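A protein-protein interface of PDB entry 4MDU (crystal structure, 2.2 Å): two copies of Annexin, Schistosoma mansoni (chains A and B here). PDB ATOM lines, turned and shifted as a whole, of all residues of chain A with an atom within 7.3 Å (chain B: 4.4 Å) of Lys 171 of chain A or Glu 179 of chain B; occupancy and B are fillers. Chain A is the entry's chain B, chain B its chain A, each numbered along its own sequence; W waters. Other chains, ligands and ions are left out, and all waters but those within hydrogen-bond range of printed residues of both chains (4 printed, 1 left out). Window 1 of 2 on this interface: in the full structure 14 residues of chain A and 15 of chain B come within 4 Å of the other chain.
Water W3 lies within hydrogen-bond range of the side-chain carboxylate (OE2) of Glu 179 of chain B (2.7 Å), the side-chain amino group (NZ) of Lys 171 of chain B (2.7 Å) and the side-chain carboxylate (OE2) of Glu 179 of chain A (3.5 Å).
Water W2 lies within hydrogen-bond range of OE2 of Glu 179 of chain A (2.8 Å) and NZ of Lys 171 of chain B (3.3 Å).
Water W4 lies within hydrogen-bond range of the backbone NH (N) of Lys 172 of chain B, the side-chain sulfur (SG) of Cys 175 of chain B and the backbone carbonyl oxygen (O) of Thr 174 of chain A.
Water W1 lies within hydrogen-bond range of the side-chain amino group of Lys 171 of chain A, the backbone NH of Tyr 178 of chain B and the side-chain carboxylate of Glu 179 of chain B.
Among the printed residues, 5 pairs touch across the chains.
Among the printed residues, Asp or Glu carboxylates within 4 Å of a Lys or Arg side-chain nitrogen of the other chain: Lys 171 of chain A with Glu 179 of chain B (2.8 Å).
The side-chain carboxylate (OE2) of Glu 179 of chain B lies within salt-bridge range of the side-chain amino group (NZ) of Lys 171 of chain A (2.8 Å).
SG of Cys 175 of chain B forms a disulfide with SG of Cys 175 of chain A, at 2.0 Å.
The backbone NH of Gly 125 of chain A sits at hydrogen-bond distance from the side-chain carboxylate of Asp 177 of chain B, at 2.8 Å.
Lys 171 of chain A touches Cys 175 of chain B, and with the chains exchanged Cys 175 of chain A touches Lys 171 of chain B.
Lys 171 of chain A touches Glu 179 of chain B, but with the chains exchanged Glu 179 of chain A does not touch Lys 171 of chain B (4.5 Å).
Cys 175 of chain B touches its own counterpart, Cys 175 of chain A.
Positions printed for both chains: 171, 172, 175, 176, 178, 179, 180, 182 and 183.
Among the printed residues, pairs that only touch across the chains: Cys 175 of chain A with Lys 171 of chain B (2.8 Å) and Lys 171 of chain A with Cys 175 of chain B (3.0 Å).
Printed residues of chain B within 4 Å of Gly 125 of chain A: Asp 177.
Of chain B, only Cys 175 (3.0 Å) and Glu 179 (2.8 Å) come within 4 Å of Lys 171 of chain A.
Glu 173 of chain A touches none of the printed residues of chain B.
Of the printed residues of chain B, Cys 175 of chain A touches Lys 171 (2.8 Å) and Cys 175 (2.0 Å).
Of the printed residues of chain A, Lys 171 of chain B touches Cys 175 (2.8 Å).
Of the printed residues of chain A, Cys 175 of chain B touches Lys 171 and Cys 175.
No residue of chain A comes within 4 Å of Gly 176 of chain B.
Of the printed residues of chain A, Asp 177 of chain B touches Gly 125 (2.8 Å).
Glu 179 of chain B touches one residue of chain A.
The nearest residue of chain A that does not touch Glu 179 of chain B is Glu 179 of chain A (4.5 Å).
The side-chain carboxylate (OE1) of Glu 179 of chain B lies close to the backbone NH (N) of Gly 176 of chain B, at 3.1 Å.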
ATOM      1  N   MET A 121      29.015  30.027 -17.407  1.00  0.00           N
ATOM      2  CA  MET A 121      27.862  29.132 -17.325  1.00  0.00           C
ATOM      3  C   MET A 121      26.515  29.859 -17.298  1.00  0.00           C
ATOM      4  O   MET A 121      25.544  29.386 -17.873  1.00  0.00           O
ATOM      5  CB  MET A 121      28.012  28.182 -16.133  1.00  0.00           C
ATOM      6  CG  MET A 121      29.218  27.245 -16.260  1.00  0.00           C
ATOM      7  SD  MET A 121      29.406  26.131 -14.861  1.00  0.00           S
ATOM      8  CE  MET A 121      29.777  27.272 -13.532  1.00  0.00           C
ATOM      9  N   GLY A 125      24.198  29.327 -23.621  1.00  0.00           N
ATOM     10  CA  GLY A 125      25.209  28.354 -23.976  1.00  0.00           C
ATOM     11  C   GLY A 125      26.216  28.285 -22.843  1.00  0.00           C
ATOM     12  O   GLY A 125      26.001  28.854 -21.768  1.00  0.00           O
ATOM     13  N   THR A 126      27.320  27.596 -23.097  1.00  0.00           N
ATOM     14  CA  THR A 126      28.328  27.328 -22.092  1.00  0.00           C
ATOM     15  C   THR A 126      29.687  27.652 -22.653  1.00  0.00           C
ATOM     16  O   THR A 126      30.054  27.148 -23.708  1.00  0.00           O
ATOM     17  CB  THR A 126      28.329  25.844 -21.717  1.00  0.00           C
ATOM     18  OG1 THR A 126      27.063  25.522 -21.132  1.00  0.00           O
ATOM     19  CG2 THR A 126      29.409  25.579 -20.718  1.00  0.00           C
ATOM     20  N   ASP A 128      32.725  26.606 -22.673  1.00  0.00           N
ATOM     21  CA  ASP A 128      33.467  25.438 -22.245  1.00  0.00           C
ATOM     22  C   ASP A 128      34.953  25.655 -22.338  1.00  0.00           C
ATOM     23  O   ASP A 128      35.728  25.123 -21.529  1.00  0.00           O
ATOM     24  CB  ASP A 128      33.045  24.230 -23.056  1.00  0.00           C
ATOM     25  CG  ASP A 128      31.761  23.630 -22.532  1.00  0.00           C
ATOM     26  OD1 ASP A 128      31.774  23.154 -21.374  1.00  0.00           O
ATOM     27  OD2 ASP A 128      30.741  23.659 -23.251  1.00  0.00           O
ATOM     28  N   LEU A 131      35.897  26.867 -19.205  1.00  0.00           N
ATOM     29  CA  LEU A 131      35.895  25.820 -18.167  1.00  0.00           C
ATOM     30  C   LEU A 131      37.159  24.965 -18.287  1.00  0.00           C
ATOM     31  O   LEU A 131      37.866  24.737 -17.306  1.00  0.00           O
ATOM     32  CB  LEU A 131      34.653  24.927 -18.262  1.00  0.00           C
ATOM     33  CG  LEU A 131      33.293  25.594 -18.240  1.00  0.00           C
ATOM     34  CD1 LEU A 131      32.152  24.539 -18.047  1.00  0.00           C
ATOM     35  CD2 LEU A 131      33.281  26.653 -17.169  1.00  0.00           C
ATOM     36  N   LEU A 166      28.996  25.459  -7.330  1.00  0.00           N
ATOM     37  CA  LEU A 166      29.665  25.328  -8.621  1.00  0.00           C
ATOM     38  C   LEU A 166      29.194  24.076  -9.350  1.00  0.00           C
ATOM     39  O   LEU A 166      28.838  24.137 -10.518  1.00  0.00           O
ATOM     40  CB  LEU A 166      31.196  25.331  -8.463  1.00  0.00           C
ATOM     41  CG  LEU A 166      32.047  25.132  -9.732  1.00  0.00           C
ATOM     42  CD1 LEU A 166      31.791  26.244 -10.764  1.00  0.00           C
ATOM     43  CD2 LEU A 166      33.533  25.063  -9.404  1.00  0.00           C
ATOM     44  N   VAL A 167      29.193  22.932  -8.674  1.00  0.00           N
ATOM     45  CA  VAL A 167      28.773  21.696  -9.340  1.00  0.00           C
ATOM     46  C   VAL A 167      27.302  21.713  -9.762  1.00  0.00           C
ATOM     47  O   VAL A 167      26.939  21.174 -10.811  1.00  0.00           O
ATOM     48  CB  VAL A 167      29.058  20.432  -8.489  1.00  0.00           C
ATOM     49  CG1 VAL A 167      28.564  19.206  -9.217  1.00  0.00           C
ATOM     50  CG2 VAL A 167      30.543  20.295  -8.216  1.00  0.00           C
ATOM     51  N   THR A 168      26.462  22.343  -8.949  1.00  0.00           N
ATOM     52  CA  THR A 168      25.057  22.521  -9.313  1.00  0.00           C
ATOM     53  C   THR A 168      24.924  23.135 -10.697  1.00  0.00           C
ATOM     54  O   THR A 168      24.052  22.759 -11.480  1.00  0.00           O
ATOM     55  CB  THR A 168      24.321  23.480  -8.360  1.00  0.00           C
ATOM     56  OG1 THR A 168      24.788  23.313  -7.019  1.00  0.00           O
ATOM     57  CG2 THR A 168      22.830  23.232  -8.427  1.00  0.00           C
ATOM     58  N   ASP A 169      25.782  24.103 -10.981  1.00  0.00           N
ATOM     59  CA  ASP A 169      25.675  24.871 -12.218  1.00  0.00           C
ATOM     60  C   ASP A 169      26.257  24.140 -13.425  1.00  0.00           C
ATOM     61  O   ASP A 169      25.853  24.375 -14.576  1.00  0.00           O
ATOM     62  CB  ASP A 169      26.337  26.233 -12.037  1.00  0.00           C
ATOM     63  CG  ASP A 169      25.470  27.187 -11.243  1.00  0.00           C
ATOM     64  OD1 ASP A 169      24.300  26.839 -10.996  1.00  0.00           O
ATOM     65  OD2 ASP A 169      25.940  28.284 -10.885  1.00  0.00           O
ATOM     66  N   MET A 170      27.199  23.246 -13.163  1.00  0.00           N
ATOM     67  CA  MET A 170      27.819  22.484 -14.235  1.00  0.00           C
ATOM     68  C   MET A 170      26.861  21.506 -14.874  1.00  0.00           C
ATOM     69  O   MET A 170      25.825  21.173 -14.306  1.00  0.00           O
ATOM     70  CB  MET A 170      29.051  21.743 -13.720  1.00  0.00           C
ATOM     71  CG  MET A 170      30.112  22.724 -13.278  1.00  0.00           C
ATOM     72  SD  MET A 170      31.578  21.944 -12.660  1.00  0.00           S
ATOM     73  CE  MET A 170      32.146  21.052 -14.114  1.00  0.00           C
ATOM     74  N   LYS A 171      27.222  21.049 -16.065  1.00  0.00           N
ATOM     75  CA  LYS A 171      26.485  19.992 -16.719  1.00  0.00           C
ATOM     76  C   LYS A 171      26.694  18.665 -15.966  1.00  0.00           C
ATOM     77  O   LYS A 171      27.766  18.416 -15.403  1.00  0.00           O
ATOM     78  CB  LYS A 171      26.927  19.886 -18.177  1.00  0.00           C
ATOM     79  CG  LYS A 171      26.556  21.112 -19.019  1.00  0.00           C
ATOM     80  CD  LYS A 171      26.810  20.899 -20.515  1.00  0.00           C
ATOM     81  CE  LYS A 171      26.373  22.136 -21.324  1.00  0.00           C
ATOM     82  NZ  LYS A 171      26.797  22.136 -22.767  1.00  0.00           N
ATOM     83  N   LYS A 172      25.659  17.829 -15.945  1.00  0.00           N
ATOM     84  CA  LYS A 172      25.722  16.532 -15.280  1.00  0.00           C
ATOM     85  C   LYS A 172      26.518  15.512 -16.091  1.00  0.00           C
ATOM     86  O   LYS A 172      26.578  15.584 -17.313  1.00  0.00           O
ATOM     87  N   GLU A 173      27.110  14.552 -15.392  1.00  0.00           N
ATOM     88  CA  GLU A 173      28.049  13.598 -15.978  1.00  0.00           C
ATOM     89  C   GLU A 173      27.409  12.688 -17.005  1.00  0.00           C
ATOM     90  O   GLU A 173      28.096  12.099 -17.837  1.00  0.00           O
ATOM     91  CB  GLU A 173      28.718  12.776 -14.879  1.00  0.00           C
ATOM     92  CG  GLU A 173      27.782  12.356 -13.762  1.00  0.00           C
ATOM     93  CD  GLU A 173      28.490  12.303 -12.418  1.00  0.00           C
ATOM     94  OE1 GLU A 173      28.941  11.203 -12.024  1.00  0.00           O
ATOM     95  OE2 GLU A 173      28.603  13.363 -11.761  1.00  0.00           O
ATOM     96  N   THR A 174      26.086  12.595 -16.951  1.00  0.00           N
ATOM     97  CA  THR A 174      25.324  11.828 -17.930  1.00  0.00           C
ATOM     98  C   THR A 174      25.248  12.541 -19.288  1.00  0.00           C
ATOM     99  O   THR A 174      24.805  11.970 -20.289  1.00  0.00           O
ATOM    100  CB  THR A 174      23.898  11.568 -17.416  1.00  0.00           C
ATOM    101  OG1 THR A 174      23.282  12.820 -17.088  1.00  0.00           O
ATOM    102  CG2 THR A 174      23.922  10.681 -16.168  1.00  0.00           C
ATOM    103  N   CYS A 175      25.671  13.796 -19.322  1.00  0.00           N
ATOM    104  CA  CYS A 175      25.635  14.549 -20.564  1.00  0.00           C
ATOM    105  C   CYS A 175      26.748  14.115 -21.530  1.00  0.00           C
ATOM    106  O   CYS A 175      26.748  14.490 -22.702  1.00  0.00           O
ATOM    107  CB  CYS A 175      25.680  16.055 -20.279  1.00  0.00           C
ATOM    108  SG  CYS A 175      24.183  16.674 -19.433  1.00  0.00           S
ATOM    109  N   GLY A 176      27.689  13.313 -21.045  1.00  0.00           N
ATOM    110  CA  GLY A 176      28.742  12.802 -21.909  1.00  0.00           C
ATOM    111  C   GLY A 176      30.129  12.685 -21.299  1.00  0.00           C
ATOM    112  O   GLY A 176      30.362  13.067 -20.148  1.00  0.00           O
ATOM    113  N   TYR A 178      32.850  14.314 -21.910  1.00  0.00           N
ATOM    114  CA  TYR A 178      33.485  15.583 -21.577  1.00  0.00           C
ATOM    115  C   TYR A 178      32.988  16.066 -20.223  1.00  0.00           C
ATOM    116  O   TYR A 178      33.778  16.485 -19.373  1.00  0.00           O
ATOM    117  CB  TYR A 178      33.210  16.637 -22.655  1.00  0.00           C
ATOM    118  CG  TYR A 178      33.442  18.074 -22.204  1.00  0.00           C
ATOM    119  CD1 TYR A 178      34.713  18.513 -21.839  1.00  0.00           C
ATOM    120  CD2 TYR A 178      32.392  18.991 -22.173  1.00  0.00           C
ATOM    121  CE1 TYR A 178      34.924  19.815 -21.434  1.00  0.00           C
ATOM    122  CE2 TYR A 178      32.593  20.310 -21.773  1.00  0.00           C
ATOM    123  CZ  TYR A 178      33.861  20.712 -21.408  1.00  0.00           C
ATOM    124  OH  TYR A 178      34.077  22.011 -21.012  1.00  0.00           O
ATOM    125  N   GLU A 179      31.677  15.989 -20.022  1.00  0.00           N
ATOM    126  CA  GLU A 179      31.054  16.495 -18.802  1.00  0.00           C
ATOM    127  C   GLU A 179      31.506  15.698 -17.589  1.00  0.00           C
ATOM    128  O   GLU A 179      31.781  16.248 -16.517  1.00  0.00           O
ATOM    129  CB  GLU A 179      29.530  16.454 -18.921  1.00  0.00           C
ATOM    130  CG  GLU A 179      28.947  17.457 -19.898  1.00  0.00           C
ATOM    131  CD  GLU A 179      29.144  17.057 -21.353  1.00  0.00           C
ATOM    132  OE1 GLU A 179      29.630  15.931 -21.590  1.00  0.00           O
ATOM    133  OE2 GLU A 179      28.803  17.864 -22.256  1.00  0.00           O
ATOM    134  N   TYR A 180      31.586  14.389 -17.769  1.00  0.00           N
ATOM    135  CA  TYR A 180      32.015  13.524 -16.692  1.00  0.00           C
ATOM    136  C   TYR A 180      33.455  13.863 -16.312  1.00  0.00           C
ATOM    137  O   TYR A 180      33.771  14.017 -15.122  1.00  0.00           O
ATOM    138  CB  TYR A 180      31.870  12.057 -17.096  1.00  0.00           C
ATOM    139  CG  TYR A 180      32.317  11.091 -16.020  1.00  0.00           C
ATOM    140  CD1 TYR A 180      33.663  10.769 -15.873  1.00  0.00           C
ATOM    141  CD2 TYR A 180      31.402  10.509 -15.147  1.00  0.00           C
ATOM    142  CE1 TYR A 180      34.090   9.897 -14.889  1.00  0.00           C
ATOM    143  CE2 TYR A 180      31.820   9.616 -14.154  1.00  0.00           C
ATOM    144  CZ  TYR A 180      33.170   9.315 -14.032  1.00  0.00           C
ATOM    145  OH  TYR A 180      33.622   8.441 -13.061  1.00  0.00           O
ATOM    146  N   LEU A 182      35.033  16.657 -16.874  1.00  0.00           N
ATOM    147  CA  LEU A 182      35.001  17.998 -16.290  1.00  0.00           C
ATOM    148  C   LEU A 182      34.683  17.908 -14.799  1.00  0.00           C
ATOM    149  O   LEU A 182      35.388  18.485 -13.971  1.00  0.00           O
ATOM    150  CB  LEU A 182      33.953  18.855 -17.003  1.00  0.00           C
ATOM    151  CG  LEU A 182      34.268  20.331 -17.251  1.00  0.00           C
ATOM    152  CD1 LEU A 182      35.639  20.473 -17.846  1.00  0.00           C
ATOM    153  CD2 LEU A 182      33.208  20.965 -18.176  1.00  0.00           C
ATOM    154  N   LEU A 183      33.624  17.168 -14.470  1.00  0.00           N
ATOM    155  CA  LEU A 183      33.228  16.915 -13.077  1.00  0.00           C
ATOM    156  C   LEU A 183      34.313  16.259 -12.229  1.00  0.00           C
ATOM    157  O   LEU A 183      34.416  16.536 -11.035  1.00  0.00           O
ATOM    158  CB  LEU A 183      31.971  16.042 -13.014  1.00  0.00           C
ATOM    159  CG  LEU A 183      30.611  16.712 -12.804  1.00  0.00           C
ATOM    160  CD1 LEU A 183      30.758  18.133 -12.259  1.00  0.00           C
ATOM    161  CD2 LEU A 183      29.818  16.701 -14.097  1.00  0.00           C
ATOM    162  N   ASP A 275      34.977  18.383 -27.184  1.00  0.00           N
ATOM    163  CA  ASP A 275      35.543  19.026 -26.012  1.00  0.00           C
ATOM    164  C   ASP A 275      36.236  18.030 -25.106  1.00  0.00           C
ATOM    165  O   ASP A 275      37.143  18.393 -24.345  1.00  0.00           O
ATOM    166  CB  ASP A 275      34.461  19.785 -25.255  1.00  0.00           C
ATOM    167  CG  ASP A 275      34.196  21.146 -25.865  1.00  0.00           C
ATOM    168  OD1 ASP A 275      35.130  21.698 -26.489  1.00  0.00           O
ATOM    169  OD2 ASP A 275      33.066  21.659 -25.737  1.00  0.00           O
ATOM    170  N   LYS B 171      22.353  13.768 -26.535  1.00  0.00           N
ATOM    171  CA  LYS B 171      22.326  14.322 -25.192  1.00  0.00           C
ATOM    172  C   LYS B 171      20.939  14.883 -24.864  1.00  0.00           C
ATOM    173  O   LYS B 171      20.202  15.291 -25.763  1.00  0.00           O
ATOM    174  CB  LYS B 171      23.400  15.402 -25.055  1.00  0.00           C
ATOM    175  CG  LYS B 171      24.797  14.915 -25.431  1.00  0.00           C
ATOM    176  CD  LYS B 171      25.870  15.899 -24.987  1.00  0.00           C
ATOM    177  CE  LYS B 171      27.112  15.825 -25.876  1.00  0.00           C
ATOM    178  NZ  LYS B 171      27.158  16.941 -26.885  1.00  0.00           N
ATOM    179  N   LYS B 172      20.584  14.896 -23.579  1.00  0.00           N
ATOM    180  CA  LYS B 172      19.250  15.332 -23.159  1.00  0.00           C
ATOM    181  C   LYS B 172      19.131  16.846 -23.157  1.00  0.00           C
ATOM    182  O   LYS B 172      20.111  17.552 -22.925  1.00  0.00           O
ATOM    183  CB  LYS B 172      18.892  14.767 -21.776  1.00  0.00           C
ATOM    184  CG  LYS B 172      18.764  13.248 -21.749  1.00  0.00           C
ATOM    185  CD  LYS B 172      18.439  12.746 -20.360  1.00  0.00           C
ATOM    186  N   CYS B 175      20.751  18.992 -20.601  1.00  0.00           N
ATOM    187  CA  CYS B 175      22.189  19.232 -20.633  1.00  0.00           C
ATOM    188  C   CYS B 175      22.539  20.681 -20.957  1.00  0.00           C
ATOM    189  O   CYS B 175      23.597  21.163 -20.565  1.00  0.00           O
ATOM    190  CB  CYS B 175      22.880  18.270 -21.591  1.00  0.00           C
ATOM    191  SG  CYS B 175      22.850  16.557 -20.971  1.00  0.00           S
ATOM    192  N   GLY B 176      21.646  21.379 -21.660  1.00  0.00           N
ATOM    193  CA  GLY B 176      21.851  22.799 -21.910  1.00  0.00           C
ATOM    194  C   GLY B 176      21.205  23.394 -23.150  1.00  0.00           C
ATOM    195  O   GLY B 176      20.556  22.703 -23.946  1.00  0.00           O
ATOM    196  N   ASP B 177      21.402  24.697 -23.316  1.00  0.00           N
ATOM    197  CA  ASP B 177      20.862  25.427 -24.451  1.00  0.00           C
ATOM    198  C   ASP B 177      21.226  24.770 -25.789  1.00  0.00           C
ATOM    199  O   ASP B 177      20.357  24.549 -26.635  1.00  0.00           O
ATOM    200  CB  ASP B 177      21.354  26.869 -24.398  1.00  0.00           C
ATOM    201  CG  ASP B 177      20.994  27.547 -23.094  1.00  0.00           C
ATOM    202  OD1 ASP B 177      19.817  27.419 -22.701  1.00  0.00           O
ATOM    203  OD2 ASP B 177      21.873  28.194 -22.469  1.00  0.00           O
ATOM    204  N   TYR B 178      22.499  24.432 -25.964  1.00  0.00           N
ATOM    205  CA  TYR B 178      22.953  23.813 -27.212  1.00  0.00           C
ATOM    206  C   TYR B 178      22.220  22.513 -27.438  1.00  0.00           C
ATOM    207  O   TYR B 178      21.674  22.265 -28.511  1.00  0.00           O
ATOM    208  CB  TYR B 178      24.463  23.557 -27.168  1.00  0.00           C
ATOM    209  CG  TYR B 178      24.995  22.545 -28.187  1.00  0.00           C
ATOM    210  CD1 TYR B 178      24.943  22.804 -29.550  1.00  0.00           C
ATOM    211  CD2 TYR B 178      25.591  21.347 -27.775  1.00  0.00           C
ATOM    212  CE1 TYR B 178      25.449  21.904 -30.483  1.00  0.00           C
ATOM    213  CE2 TYR B 178      26.102  20.430 -28.706  1.00  0.00           C
ATOM    214  CZ  TYR B 178      26.030  20.726 -30.062  1.00  0.00           C
ATOM    215  OH  TYR B 178      26.524  19.845 -31.002  1.00  0.00           O
ATOM    216  N   GLU B 179      22.202  21.674 -26.412  1.00  0.00           N
ATOM    217  CA  GLU B 179      21.586  20.368 -26.548  1.00  0.00           C
ATOM    218  C   GLU B 179      20.079  20.480 -26.823  1.00  0.00           C
ATOM    219  O   GLU B 179      19.517  19.696 -27.602  1.00  0.00           O
ATOM    220  CB  GLU B 179      21.887  19.515 -25.312  1.00  0.00           C
ATOM    221  CG  GLU B 179      23.373  19.237 -25.106  1.00  0.00           C
ATOM    222  CD  GLU B 179      24.133  20.344 -24.362  1.00  0.00           C
ATOM    223  OE1 GLU B 179      23.581  21.450 -24.143  1.00  0.00           O
ATOM    224  OE2 GLU B 179      25.300  20.092 -23.982  1.00  0.00           O
ATOM    225  N   TYR B 180      19.429  21.469 -26.211  1.00  0.00           N
ATOM    226  CA  TYR B 180      17.999  21.691 -26.450  1.00  0.00           C
ATOM    227  C   TYR B 180      17.751  22.134 -27.883  1.00  0.00           C
ATOM    228  O   TYR B 180      16.780  21.713 -28.531  1.00  0.00           O
ATOM    229  CB  TYR B 180      17.455  22.743 -25.481  1.00  0.00           C
ATOM    230  CG  TYR B 180      16.039  23.203 -25.783  1.00  0.00           C
ATOM    231  CD1 TYR B 180      15.794  24.192 -26.730  1.00  0.00           C
ATOM    232  CD2 TYR B 180      14.948  22.656 -25.109  1.00  0.00           C
ATOM    233  CE1 TYR B 180      14.502  24.623 -27.005  1.00  0.00           C
ATOM    234  CE2 TYR B 180      13.650  23.081 -25.374  1.00  0.00           C
ATOM    235  CZ  TYR B 180      13.433  24.066 -26.323  1.00  0.00           C
ATOM    236  OH  TYR B 180      12.150  24.493 -26.592  1.00  0.00           O
ATOM    237  N   ALA B 181      18.621  23.011 -28.374  1.00  0.00           N
ATOM    238  CA  ALA B 181      18.495  23.503 -29.747  1.00  0.00           C
ATOM    239  C   ALA B 181      18.672  22.349 -30.729  1.00  0.00           C
ATOM    240  O   ALA B 181      17.959  22.238 -31.723  1.00  0.00           O
ATOM    241  CB  ALA B 181      19.518  24.576 -30.007  1.00  0.00           C
ATOM    242  N   LEU B 182      19.624  21.480 -30.423  1.00  0.00           N
ATOM    243  CA  LEU B 182      19.897  20.319 -31.255  1.00  0.00           C
ATOM    244  C   LEU B 182      18.662  19.451 -31.329  1.00  0.00           C
ATOM    245  O   LEU B 182      18.310  18.949 -32.389  1.00  0.00           O
ATOM    246  CB  LEU B 182      21.044  19.515 -30.654  1.00  0.00           C
ATOM    247  CG  LEU B 182      22.190  19.123 -31.583  1.00  0.00           C
ATOM    248  CD1 LEU B 182      22.642  20.302 -32.432  1.00  0.00           C
ATOM    249  CD2 LEU B 182      23.333  18.562 -30.751  1.00  0.00           C
ATOM    250  N   LEU B 183      18.012  19.270 -30.185  1.00  0.00           N
ATOM    251  CA  LEU B 183      16.834  18.423 -30.102  1.00  0.00           C
ATOM    252  C   LEU B 183      15.695  19.112 -30.854  1.00  0.00           C
ATOM    253  O   LEU B 183      14.930  18.465 -31.566  1.00  0.00           O
ATOM    254  CB  LEU B 183      16.464  18.178 -28.635  1.00  0.00           C
ATOM    255  CG  LEU B 183      16.384  16.762 -28.044  1.00  0.00           C
ATOM    256  CD1 LEU B 183      17.062  15.717 -28.909  1.00  0.00           C
ATOM    257  CD2 LEU B 183      16.949  16.735 -26.613  1.00  0.00           C
HETATM  258  O   HOH W   1      24.940  24.588 -23.798  1.00  0.00           O
HETATM  259  O   HOH W   2      29.509  16.586 -24.659  1.00  0.00           O
HETATM  260  O   HOH W   3      27.490  19.103 -25.234  1.00  0.00           O
HETATM  261  O   HOH W   4      22.188  13.420 -21.797  1.00  0.00           O
